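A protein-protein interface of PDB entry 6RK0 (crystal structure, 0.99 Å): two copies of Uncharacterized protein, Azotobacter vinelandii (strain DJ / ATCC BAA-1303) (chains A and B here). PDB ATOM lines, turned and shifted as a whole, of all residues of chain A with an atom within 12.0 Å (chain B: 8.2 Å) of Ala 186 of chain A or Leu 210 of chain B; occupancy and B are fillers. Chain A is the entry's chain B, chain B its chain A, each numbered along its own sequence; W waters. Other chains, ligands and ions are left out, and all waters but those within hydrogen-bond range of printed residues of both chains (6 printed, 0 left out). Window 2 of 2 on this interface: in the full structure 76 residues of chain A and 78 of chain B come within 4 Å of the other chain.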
ATOM      1  N   ILE A 100      22.269  19.778  -2.045  1.00  0.00           N
ATOM      2  CA  ILE A 100      21.257  19.478  -3.057  1.00  0.00           C
ATOM      3  C   ILE A 100      20.641  20.806  -3.491  1.00  0.00           C
ATOM      4  O   ILE A 100      19.942  21.468  -2.713  1.00  0.00           O
ATOM      5  CB  ILE A 100      20.195  18.543  -2.464  1.00  0.00           C
ATOM      6  CG1 ILE A 100      20.798  17.191  -2.050  1.00  0.00           C
ATOM      7  CG2 ILE A 100      19.060  18.331  -3.458  1.00  0.00           C
ATOM      8  CD1 ILE A 100      19.953  16.419  -1.121  1.00  0.00           C
ATOM      9  N   ALA A 101      20.906  21.208  -4.727  1.00  0.00           N
ATOM     10  CA  ALA A 101      20.432  22.471  -5.271  1.00  0.00           C
ATOM     11  C   ALA A 101      19.253  22.220  -6.205  1.00  0.00           C
ATOM     12  O   ALA A 101      18.895  21.083  -6.520  1.00  0.00           O
ATOM     13  CB  ALA A 101      21.549  23.170  -6.016  1.00  0.00           C
ATOM     14  N   ARG A 102      18.644  23.321  -6.670  1.00  0.00           N
ATOM     15  CA  ARG A 102      17.540  23.242  -7.623  1.00  0.00           C
ATOM     16  C   ARG A 102      18.006  22.879  -9.026  1.00  0.00           C
ATOM     17  O   ARG A 102      17.191  22.372  -9.807  1.00  0.00           O
ATOM     18  CB  ARG A 102      16.812  24.576  -7.638  1.00  0.00           C
ATOM     19  CG  ARG A 102      16.121  24.904  -6.336  1.00  0.00           C
ATOM     20  CD  ARG A 102      15.893  26.404  -6.178  1.00  0.00           C
ATOM     21  NE  ARG A 102      15.295  26.677  -4.873  1.00  0.00           N
ATOM     22  CZ  ARG A 102      15.954  26.654  -3.719  1.00  0.00           C
ATOM     23  NH1 ARG A 102      17.274  26.502  -3.674  1.00  0.00           N
ATOM     24  NH2 ARG A 102      15.299  26.852  -2.574  1.00  0.00           N
ATOM     25  N   SER A 103      19.262  23.177  -9.377  1.00  0.00           N
ATOM     26  CA  SER A 103      19.852  22.765 -10.636  1.00  0.00           C
ATOM     27  C   SER A 103      20.993  21.807 -10.349  1.00  0.00           C
ATOM     28  O   SER A 103      21.722  21.972  -9.365  1.00  0.00           O
ATOM     29  CB  SER A 103      20.329  23.940 -11.459  1.00  0.00           C
ATOM     30  OG  SER A 103      21.464  24.528 -10.907  1.00  0.00           O
ATOM     31  N   PRO A 177      23.659  26.364   3.281  1.00  0.00           N
ATOM     32  CA  PRO A 177      22.661  25.827   2.335  1.00  0.00           C
ATOM     33  C   PRO A 177      23.167  25.860   0.904  1.00  0.00           C
ATOM     34  O   PRO A 177      24.190  26.493   0.566  1.00  0.00           O
ATOM     35  CB  PRO A 177      21.470  26.789   2.511  1.00  0.00           C
ATOM     36  CG  PRO A 177      22.155  28.081   2.914  1.00  0.00           C
ATOM     37  CD  PRO A 177      23.213  27.652   3.868  1.00  0.00           C
ATOM     38  N   PRO A 178      22.413  25.238   0.005  1.00  0.00           N
ATOM     39  CA  PRO A 178      22.668  25.408  -1.430  1.00  0.00           C
ATOM     40  C   PRO A 178      22.580  26.867  -1.846  1.00  0.00           C
ATOM     41  O   PRO A 178      21.878  27.669  -1.233  1.00  0.00           O
ATOM     42  CB  PRO A 178      21.564  24.563  -2.108  1.00  0.00           C
ATOM     43  CG  PRO A 178      20.583  24.365  -1.071  1.00  0.00           C
ATOM     44  CD  PRO A 178      21.223  24.407   0.248  1.00  0.00           C
ATOM     45  N   LEU A 179      23.256  27.176  -2.952  1.00  0.00           N
ATOM     46  CA  LEU A 179      23.188  28.502  -3.565  1.00  0.00           C
ATOM     47  C   LEU A 179      22.848  28.326  -5.033  1.00  0.00           C
ATOM     48  O   LEU A 179      23.677  27.880  -5.828  1.00  0.00           O
ATOM     49  CB  LEU A 179      24.511  29.227  -3.349  1.00  0.00           C
ATOM     50  CG  LEU A 179      24.852  29.599  -1.885  1.00  0.00           C
ATOM     51  CD1 LEU A 179      26.275  30.133  -1.730  1.00  0.00           C
ATOM     52  CD2 LEU A 179      23.852  30.647  -1.374  1.00  0.00           C
ATOM     53  N   ASP A 180      21.618  28.634  -5.387  1.00  0.00           N
ATOM     54  CA  ASP A 180      21.144  28.536  -6.755  1.00  0.00           C
ATOM     55  C   ASP A 180      21.218  29.882  -7.464  1.00  0.00           C
ATOM     56  O   ASP A 180      21.289  30.953  -6.859  1.00  0.00           O
ATOM     57  CB  ASP A 180      19.713  27.992  -6.775  1.00  0.00           C
ATOM     58  CG  ASP A 180      19.684  26.473  -6.683  1.00  0.00           C
ATOM     59  OD1 ASP A 180      20.170  25.831  -7.642  1.00  0.00           O
ATOM     60  OD2 ASP A 180      19.180  25.938  -5.658  1.00  0.00           O
ATOM     61  N   ASP A 181      21.153  29.806  -8.793  1.00  0.00           N
ATOM     62  CA  ASP A 181      20.982  31.014  -9.593  1.00  0.00           C
ATOM     63  C   ASP A 181      19.701  31.718  -9.152  1.00  0.00           C
ATOM     64  O   ASP A 181      18.694  31.068  -8.861  1.00  0.00           O
ATOM     65  CB  ASP A 181      20.802  30.632 -11.066  1.00  0.00           C
ATOM     66  CG  ASP A 181      21.975  29.912 -11.670  1.00  0.00           C
ATOM     67  OD1 ASP A 181      23.086  29.903 -11.092  1.00  0.00           O
ATOM     68  OD2 ASP A 181      21.773  29.320 -12.777  1.00  0.00           O
ATOM     69  N   GLU A 182      19.731  33.056  -9.186  1.00  0.00           N
ATOM     70  CA  GLU A 182      18.611  33.829  -8.660  1.00  0.00           C
ATOM     71  C   GLU A 182      17.301  33.486  -9.359  1.00  0.00           C
ATOM     72  O   GLU A 182      16.246  33.452  -8.703  1.00  0.00           O
ATOM     73  CB  GLU A 182      18.938  35.326  -8.746  1.00  0.00           C
ATOM     74  CG  GLU A 182      19.130  35.880 -10.171  1.00  0.00           C
ATOM     75  CD  GLU A 182      19.516  37.386 -10.249  1.00  0.00           C
ATOM     76  OE1 GLU A 182      19.324  38.001 -11.323  1.00  0.00           O
ATOM     77  OE2 GLU A 182      20.043  37.979  -9.300  1.00  0.00           O
ATOM     78  N   GLU A 183      17.349  33.187 -10.663  1.00  0.00           N
ATOM     79  CA  GLU A 183      16.142  32.926 -11.438  1.00  0.00           C
ATOM     80  C   GLU A 183      15.559  31.553 -11.173  1.00  0.00           C
ATOM     81  O   GLU A 183      14.471  31.271 -11.673  1.00  0.00           O
ATOM     82  CB  GLU A 183      16.394  33.044 -12.947  1.00  0.00           C
ATOM     83  CG  GLU A 183      17.134  34.317 -13.372  1.00  0.00           C
ATOM     84  CD  GLU A 183      18.662  34.151 -13.405  1.00  0.00           C
ATOM     85  OE1 GLU A 183      19.224  33.396 -12.574  1.00  0.00           O
ATOM     86  OE2 GLU A 183      19.302  34.795 -14.269  1.00  0.00           O
ATOM     87  N   ASP A 184      16.253  30.682 -10.431  1.00  0.00           N
ATOM     88  CA  ASP A 184      15.805  29.312 -10.215  1.00  0.00           C
ATOM     89  C   ASP A 184      14.959  29.134  -8.960  1.00  0.00           C
ATOM     90  O   ASP A 184      14.441  28.033  -8.730  1.00  0.00           O
ATOM     91  CB  ASP A 184      16.996  28.354 -10.180  1.00  0.00           C
ATOM     92  CG  ASP A 184      17.661  28.191 -11.527  1.00  0.00           C
ATOM     93  OD1 ASP A 184      17.015  28.439 -12.559  1.00  0.00           O
ATOM     94  OD2 ASP A 184      18.842  27.787 -11.567  1.00  0.00           O
ATOM     95  N   TYR A 185      14.818  30.170  -8.135  1.00  0.00           N
ATOM     96  CA  TYR A 185      14.087  30.030  -6.884  1.00  0.00           C
ATOM     97  C   TYR A 185      12.588  29.871  -7.047  1.00  0.00           C
ATOM     98  O   TYR A 185      11.931  29.494  -6.070  1.00  0.00           O
ATOM     99  CB  TYR A 185      14.460  31.154  -5.905  1.00  0.00           C
ATOM    100  CG  TYR A 185      15.801  30.882  -5.256  1.00  0.00           C
ATOM    101  CD1 TYR A 185      15.888  30.169  -4.049  1.00  0.00           C
ATOM    102  CD2 TYR A 185      16.984  31.260  -5.880  1.00  0.00           C
ATOM    103  CE1 TYR A 185      17.099  29.863  -3.485  1.00  0.00           C
ATOM    104  CE2 TYR A 185      18.219  30.953  -5.331  1.00  0.00           C
ATOM    105  CZ  TYR A 185      18.275  30.229  -4.140  1.00  0.00           C
ATOM    106  OH  TYR A 185      19.502  29.914  -3.599  1.00  0.00           O
ATOM    107  N   ALA A 186      12.039  30.080  -8.243  1.00  0.00           N
ATOM    108  CA  ALA A 186      10.632  29.779  -8.468  1.00  0.00           C
ATOM    109  C   ALA A 186      10.459  28.332  -8.938  1.00  0.00           C
ATOM    110  O   ALA A 186       9.326  27.881  -9.115  1.00  0.00           O
ATOM    111  CB  ALA A 186      10.016  30.750  -9.476  1.00  0.00           C
ATOM    112  N   PHE A 187      11.554  27.577  -9.164  1.00  0.00           N
ATOM    113  CA  PHE A 187      11.400  26.238  -9.714  1.00  0.00           C
ATOM    114  C   PHE A 187      11.035  25.270  -8.593  1.00  0.00           C
ATOM    115  O   PHE A 187      11.711  25.257  -7.562  1.00  0.00           O
ATOM    116  CB  PHE A 187      12.659  25.761 -10.435  1.00  0.00           C
ATOM    117  CG  PHE A 187      12.397  24.485 -11.179  1.00  0.00           C
ATOM    118  CD1 PHE A 187      11.856  24.527 -12.454  1.00  0.00           C
ATOM    119  CD2 PHE A 187      12.598  23.249 -10.568  1.00  0.00           C
ATOM    120  CE1 PHE A 187      11.503  23.360 -13.128  1.00  0.00           C
ATOM    121  CE2 PHE A 187      12.262  22.074 -11.268  1.00  0.00           C
ATOM    122  CZ  PHE A 187      11.710  22.156 -12.527  1.00  0.00           C
ATOM    123  N   PRO A 188       9.989  24.444  -8.758  1.00  0.00           N
ATOM    124  CA  PRO A 188       9.512  23.614  -7.625  1.00  0.00           C
ATOM    125  C   PRO A 188      10.310  22.314  -7.493  1.00  0.00           C
ATOM    126  O   PRO A 188       9.875  21.222  -7.893  1.00  0.00           O
ATOM    127  CB  PRO A 188       8.048  23.345  -8.004  1.00  0.00           C
ATOM    128  CG  PRO A 188       8.085  23.307  -9.478  1.00  0.00           C
ATOM    129  CD  PRO A 188       9.039  24.398  -9.896  1.00  0.00           C
ATOM    130  N   SER A 189      11.485  22.437  -6.879  1.00  0.00           N
ATOM    131  CA  SER A 189      12.293  21.295  -6.474  1.00  0.00           C
ATOM    132  C   SER A 189      12.803  21.554  -5.066  1.00  0.00           C
ATOM    133  O   SER A 189      13.027  22.704  -4.683  1.00  0.00           O
ATOM    134  CB  SER A 189      13.431  21.062  -7.481  1.00  0.00           C
ATOM    135  OG  SER A 189      14.137  19.854  -7.259  1.00  0.00           O
ATOM    136  N   TRP A 190      12.955  20.482  -4.305  1.00  0.00           N
ATOM    137  CA  TRP A 190      13.384  20.579  -2.915  1.00  0.00           C
ATOM    138  C   TRP A 190      14.913  20.672  -2.851  1.00  0.00           C
ATOM    139  O   TRP A 190      15.609  19.797  -3.372  1.00  0.00           O
ATOM    140  CB  TRP A 190      12.935  19.324  -2.179  1.00  0.00           C
ATOM    141  CG  TRP A 190      13.153  19.331  -0.693  1.00  0.00           C
ATOM    142  CD1 TRP A 190      12.239  19.707   0.267  1.00  0.00           C
ATOM    143  CD2 TRP A 190      14.342  18.940   0.012  1.00  0.00           C
ATOM    144  NE1 TRP A 190      12.779  19.567   1.519  1.00  0.00           N
ATOM    145  CE2 TRP A 190      14.079  19.111   1.398  1.00  0.00           C
ATOM    146  CE3 TRP A 190      15.608  18.463  -0.394  1.00  0.00           C
ATOM    147  CZ2 TRP A 190      15.022  18.799   2.378  1.00  0.00           C
ATOM    148  CZ3 TRP A 190      16.530  18.176   0.591  1.00  0.00           C
ATOM    149  CH2 TRP A 190      16.244  18.349   1.955  1.00  0.00           C
ATOM    150  N   ALA A 191      15.402  21.692  -2.171  1.00  0.00           N
ATOM    151  CA  ALA A 191      16.837  21.898  -1.981  1.00  0.00           C
ATOM    152  C   ALA A 191      17.159  21.753  -0.491  1.00  0.00           C
ATOM    153  O   ALA A 191      16.301  21.925   0.377  1.00  0.00           O
ATOM    154  CB  ALA A 191      17.213  23.274  -2.517  1.00  0.00           C
ATOM    155  N   GLY A 192      18.429  21.444  -0.199  1.00  0.00           N
ATOM    156  CA  GLY A 192      18.826  21.295   1.188  1.00  0.00           C
ATOM    157  C   GLY A 192      20.196  20.656   1.275  1.00  0.00           C
ATOM    158  O   GLY A 192      20.942  20.623   0.299  1.00  0.00           O
ATOM    159  N   ARG B 149      15.576  21.639 -11.991  1.00  0.00           N
ATOM    160  CA  ARG B 149      15.379  22.640 -13.035  1.00  0.00           C
ATOM    161  C   ARG B 149      16.132  22.157 -14.273  1.00  0.00           C
ATOM    162  O   ARG B 149      17.349  21.917 -14.186  1.00  0.00           O
ATOM    163  CB  ARG B 149      15.863  24.023 -12.589  1.00  0.00           C
ATOM    164  CG  ARG B 149      15.541  25.161 -13.554  1.00  0.00           C
ATOM    165  CD  ARG B 149      16.614  25.344 -14.592  1.00  0.00           C
ATOM    166  NE  ARG B 149      17.819  25.936 -14.001  1.00  0.00           N
ATOM    167  CZ  ARG B 149      19.081  25.681 -14.348  1.00  0.00           C
ATOM    168  NH1 ARG B 149      20.061  26.381 -13.777  1.00  0.00           N
ATOM    169  NH2 ARG B 149      19.417  24.763 -15.248  1.00  0.00           N
ATOM    170  N   ASP B 206      16.557  23.630   2.687  1.00  0.00           N
ATOM    171  CA  ASP B 206      16.872  25.036   2.434  1.00  0.00           C
ATOM    172  C   ASP B 206      15.674  25.867   2.902  1.00  0.00           C
ATOM    173  O   ASP B 206      14.541  25.625   2.452  1.00  0.00           O
ATOM    174  CB  ASP B 206      17.033  25.200   0.915  1.00  0.00           C
ATOM    175  CG  ASP B 206      17.398  26.599   0.478  1.00  0.00           C
ATOM    176  OD1 ASP B 206      17.499  27.509   1.335  1.00  0.00           O
ATOM    177  OD2 ASP B 206      17.603  26.767  -0.760  1.00  0.00           O
ATOM    178  N   PRO B 207      15.882  26.871   3.749  1.00  0.00           N
ATOM    179  CA  PRO B 207      14.757  27.750   4.138  1.00  0.00           C
ATOM    180  C   PRO B 207      14.062  28.394   2.970  1.00  0.00           C
ATOM    181  O   PRO B 207      12.886  28.766   3.103  1.00  0.00           O
ATOM    182  CB  PRO B 207      15.427  28.793   5.049  1.00  0.00           C
ATOM    183  CG  PRO B 207      16.653  28.094   5.610  1.00  0.00           C
ATOM    184  CD  PRO B 207      17.117  27.176   4.493  1.00  0.00           C
ATOM    185  N   ARG B 208      14.759  28.586   1.843  1.00  0.00           N
ATOM    186  CA  ARG B 208      14.190  29.199   0.662  1.00  0.00           C
ATOM    187  C   ARG B 208      13.383  28.232  -0.197  1.00  0.00           C
ATOM    188  O   ARG B 208      12.891  28.621  -1.254  1.00  0.00           O
ATOM    189  CB  ARG B 208      15.276  29.906  -0.140  1.00  0.00           C
ATOM    190  CG  ARG B 208      15.775  31.087   0.650  1.00  0.00           C
ATOM    191  CD  ARG B 208      16.617  32.051  -0.147  1.00  0.00           C
ATOM    192  NE  ARG B 208      15.903  32.581  -1.303  1.00  0.00           N
ATOM    193  CZ  ARG B 208      16.518  33.143  -2.337  1.00  0.00           C
ATOM    194  NH1 ARG B 208      17.828  33.235  -2.328  1.00  0.00           N
ATOM    195  NH2 ARG B 208      15.812  33.581  -3.372  1.00  0.00           N
ATOM    196  N   ASN B 209      13.241  26.981   0.231  1.00  0.00           N
ATOM    197  CA  ASN B 209      12.353  26.079  -0.492  1.00  0.00           C
ATOM    198  C   ASN B 209      10.955  26.684  -0.576  1.00  0.00           C
ATOM    199  O   ASN B 209      10.465  27.339   0.362  1.00  0.00           O
ATOM    200  CB  ASN B 209      12.244  24.752   0.228  1.00  0.00           C
ATOM    201  CG  ASN B 209      13.390  23.820  -0.105  1.00  0.00           C
ATOM    202  OD1 ASN B 209      14.155  24.024  -1.048  1.00  0.00           O
ATOM    203  ND2 ASN B 209      13.503  22.766   0.693  1.00  0.00           N
ATOM    204  N   LEU B 210      10.291  26.429  -1.690  1.00  0.00           N
ATOM    205  CA  LEU B 210       8.898  26.808  -1.821  1.00  0.00           C
ATOM    206  C   LEU B 210       8.084  26.023  -0.808  1.00  0.00           C
ATOM    207  O   LEU B 210       8.336  24.833  -0.589  1.00  0.00           O
ATOM    208  CB  LEU B 210       8.396  26.548  -3.246  1.00  0.00           C
ATOM    209  CG  LEU B 210       9.026  27.461  -4.324  1.00  0.00           C
ATOM    210  CD1 LEU B 210       8.721  26.949  -5.725  1.00  0.00           C
ATOM    211  CD2 LEU B 210       8.550  28.906  -4.178  1.00  0.00           C
ATOM    212  N   PRO B 211       7.056  26.637  -0.235  1.00  0.00           N
ATOM    213  CA  PRO B 211       6.356  25.993   0.879  1.00  0.00           C
ATOM    214  C   PRO B 211       5.652  24.698   0.528  1.00  0.00           C
ATOM    215  O   PRO B 211       5.489  23.852   1.414  1.00  0.00           O
ATOM    216  CB  PRO B 211       5.393  27.078   1.377  1.00  0.00           C
ATOM    217  CG  PRO B 211       5.328  28.094   0.307  1.00  0.00           C
ATOM    218  CD  PRO B 211       6.640  28.042  -0.407  1.00  0.00           C
ATOM    219  N   ASP B 212       5.241  24.476  -0.716  1.00  0.00           N
ATOM    220  CA  ASP B 212       4.461  23.259  -0.971  1.00  0.00           C
ATOM    221  C   ASP B 212       5.247  22.147  -1.662  1.00  0.00           C
ATOM    222  O   ASP B 212       4.662  21.253  -2.284  1.00  0.00           O
ATOM    223  CB  ASP B 212       3.193  23.610  -1.745  1.00  0.00           C
ATOM    224  CG  ASP B 212       2.334  24.636  -1.014  1.00  0.00           C
ATOM    225  OD1 ASP B 212       1.941  25.648  -1.641  1.00  0.00           O
ATOM    226  OD2 ASP B 212       2.050  24.432   0.190  1.00  0.00           O
ATOM    227  N   VAL B 213       6.560  22.170  -1.550  1.00  0.00           N
ATOM    228  CA  VAL B 213       7.427  21.257  -2.282  1.00  0.00           C
ATOM    229  C   VAL B 213       8.027  20.289  -1.272  1.00  0.00           C
ATOM    230  O   VAL B 213       8.929  20.665  -0.507  1.00  0.00           O
ATOM    231  CB  VAL B 213       8.508  22.033  -3.039  1.00  0.00           C
ATOM    232  CG1 VAL B 213       9.479  21.071  -3.688  1.00  0.00           C
ATOM    233  CG2 VAL B 213       7.844  22.915  -4.095  1.00  0.00           C
ATOM    234  N   PRO B 214       7.582  19.048  -1.233  1.00  0.00           N
ATOM    235  CA  PRO B 214       8.088  18.125  -0.211  1.00  0.00           C
ATOM    236  C   PRO B 214       9.432  17.519  -0.590  1.00  0.00           C
ATOM    237  O   PRO B 214       9.834  17.486  -1.753  1.00  0.00           O
ATOM    238  CB  PRO B 214       7.022  17.029  -0.186  1.00  0.00           C
ATOM    239  CG  PRO B 214       6.502  17.026  -1.578  1.00  0.00           C
ATOM    240  CD  PRO B 214       6.463  18.460  -1.997  1.00  0.00           C
ATOM    241  N   MET B 215      10.104  17.008   0.427  1.00  0.00           N
ATOM    242  CA  MET B 215      11.377  16.324   0.202  1.00  0.00           C
ATOM    243  C   MET B 215      11.121  14.970  -0.441  1.00  0.00           C
ATOM    244  O   MET B 215      10.352  14.162   0.105  1.00  0.00           O
ATOM    245  CB  MET B 215      12.079  16.104   1.516  1.00  0.00           C
ATOM    246  CG  MET B 215      13.449  15.430   1.309  1.00  0.00           C
ATOM    247  SD  MET B 215      14.257  14.956   2.839  1.00  0.00           S
ATOM    248  CE  MET B 215      13.368  13.440   3.212  1.00  0.00           C
HETATM  249  O   HOH W   1      15.985  34.778  -6.186  1.00  0.00           O
HETATM  250  O   HOH W   2      18.486  29.297 -14.754  1.00  0.00           O
HETATM  251  O   HOH W   3      11.689  24.997  -3.711  1.00  0.00           O
HETATM  252  O   HOH W   4      12.045  30.413  -3.180  1.00  0.00           O
HETATM  253  O   HOH W   5      20.883  32.344  -3.225  1.00  0.00           O
HETATM  254  O   HOH W   6      19.396  28.740  -1.273  1.00  0.00           O
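Ile 100 of chain A touches none of the printed residues of chain B.
Printed residues of chain B within 4 Å of Pro 178 of chain A: Asp 206.
Glu 183 of chain A touches none of the printed residues of chain B.
Printed residues of chain B within 4 Å of Tyr 185 of chain A: Arg 208 and Leu 210.
Ala 186 of chain A touches just one residue of chain B: Leu 210 (3.6 Å).
Printed residues of chain B within 4 Å of Ala 191 of chain A: Asp 206 and Asn 209.
Of the printed residues of chain B, Gly 192 of chain A touches Asp 206.
Of chain A, only Arg 102 (3.4 Å), Trp 190 (3.3 Å) and Ala 191 (2.9 Å) come within 4 Å of Asn 209 of chain B.
Leu 210 of chain B touches four residues of chain A.
No residue of chain A comes within 4 Å of Pro 211 of chain B.
No residue of chain A comes within 4 Å of Asp 212 of chain B.
Of chain A, only Pro 188 (3.9 Å), Ser 189 (3.6 Å) and Trp 190 (3.5 Å) come within 4 Å of Val 213 of chain B.
Printed residues of chain A within 4 Å of Pro 214 of chain B: Trp 190.
The nearest residue of chain B that does not touch Ala 186 of chain A is Arg 208 of chain B (7.1 Å).
The nearest printed residue of chain A that does not touch Pro 214 of chain B is Ser 189 of chain A (6.0 Å).
No position is printed for both chains.
Of the 23 pairs that touch across the chains among the printed residues, none has its exchanged pair printed and touching as well.
The backbone carbonyl oxygen (O) of Ala 191 of chain A is in hydrogen-bond range of the backbone NH (N) of Asp 206 of chain B.
OD1 of Asn 209 of chain B sits at hydrogen-bond distance from NH2 of Arg 102 of chain A (3.4 Å).
The guanidinium group (NH1) of Arg 149 of chain B lies within salt-bridge range of the side-chain carboxylate (OD2) of Asp 184 of chain A (2.9 Å).
NE1 of Trp 190 of chain A sits close to ND2 of Asn 209 of chain B (3.4 Å).
The backbone carbonyl oxygen (O) of Arg 208 of chain B sits at hydrogen-bond distance from the guanidinium group (NH2) of Arg 102 of chain A (3.3 Å).
NH2 of Arg 102 of chain A is in salt-bridge range of OD2 of Asp 206 of chain B (2.9 Å).
The side-chain carboxylate (OD2) of Asp 181 of chain A lies within salt-bridge range of the guanidinium group (NH1) of Arg 149 of chain B, at 3.5 Å.
The side-chain amide oxygen of Asn 209 of chain B is in hydrogen-bond range of the backbone NH of Ala 191 of chain A (2.9 Å).
N of Arg 149 of chain B lies within hydrogen-bond range of O of Arg 102 of chain A (2.8 Å).
Arg 149 of chain B touches Ser 103 of chain A (NH1 to CB, 3.4 Å).
Tyr 185 of chain A touches Arg 208 of chain B.
Tyr 185 of chain A touches Leu 210 of chain B.
N of Arg 149 of chain B touches CE2 of Phe 187 of chain A, at 3.4 Å.
Phe 187 of chain A touches Leu 210 of chain B.
Pro 188 of chain A touches Leu 210 of chain B.
Val 213 of chain B touches Ser 189 of chain A.
Trp 190 of chain A touches Pro 214 of chain B.
Met 215 of chain B touches Trp 190 of chain A (N to CD1, 3.4 Å).
Asp 206 of chain B touches Gly 192 of chain A.
Hydrophobic or aromatic side chains of chain A within 4 Å of the printed part of chain B: Pro 178, Tyr 185, Phe 187, Pro 188, Trp 190 and Ala 191.
Along chain A the printed residues that touch a printed residue of chain B span positions 102 to 192.
Of the 11 printed residues of chain B, 8 touch a printed residue of chain A.
Among the printed residues, 23 pairs touch across the chains.
Among the printed residues, Asp or Glu carboxylates within 4 Å of a Lys or Arg side-chain nitrogen of the other chain: Arg 102 of chain A with Asp 206 of chain B (2.9 Å), Asp 181 of chain A with Arg 149 of chain B (3.5 Å) and Asp 184 of chain A with Arg 149 of chain B (2.9 Å).
The side-chain carboxylate (OD1) of Asp 206 of chain B is in hydrogen-bond range of the backbone NH (N) of Arg 208 of chain B, 3.0 Å away.
OD2 of Asp 180 of chain A lies within salt-bridge range of NH1 of Arg 102 of chain A (2.8 Å).
N of Ser 103 of chain A sits at hydrogen-bond distance from OD1 of Asp 180 of chain A.
N of Asp 180 of chain A lies within hydrogen-bond range of OH of Tyr 185 of chain A (3.1 Å).
O of Gly 192 of chain A is in hydrogen-bond range of N of Ile 100 of chain A, 2.8 Å away.
Water W6 lies within hydrogen-bond range of OH of Tyr 185 of chain A, O of Pro 178 of chain A and OD2 of Asp 206 of chain B.
Water W4 lies within hydrogen-bond range of the backbone carbonyl oxygen (O) of Arg 208 of chain B (2.8 Å) and the backbone carbonyl oxygen (O) of Tyr 185 of chain A (3.0 Å).
Water W2 lies within hydrogen-bond range of OD1 of Asp 184 of chain A (2.8 Å) and NH1 of Arg 149 of chain B (3.5 Å).
Water W5 lies within hydrogen-bond range of OH of Tyr 185 of chain A and NH1 of Arg 208 of chain B.
Water W3 lies within hydrogen-bond range of the backbone carbonyl oxygen of Ser 189 of chain A (2.8 Å) and the backbone NH of Leu 210 of chain B (2.8 Å).
Water W1 bridges the backbone carbonyl oxygen (O) of Glu 182 of chain A and the guanidinium group (NH2) of Arg 208 of chain B.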
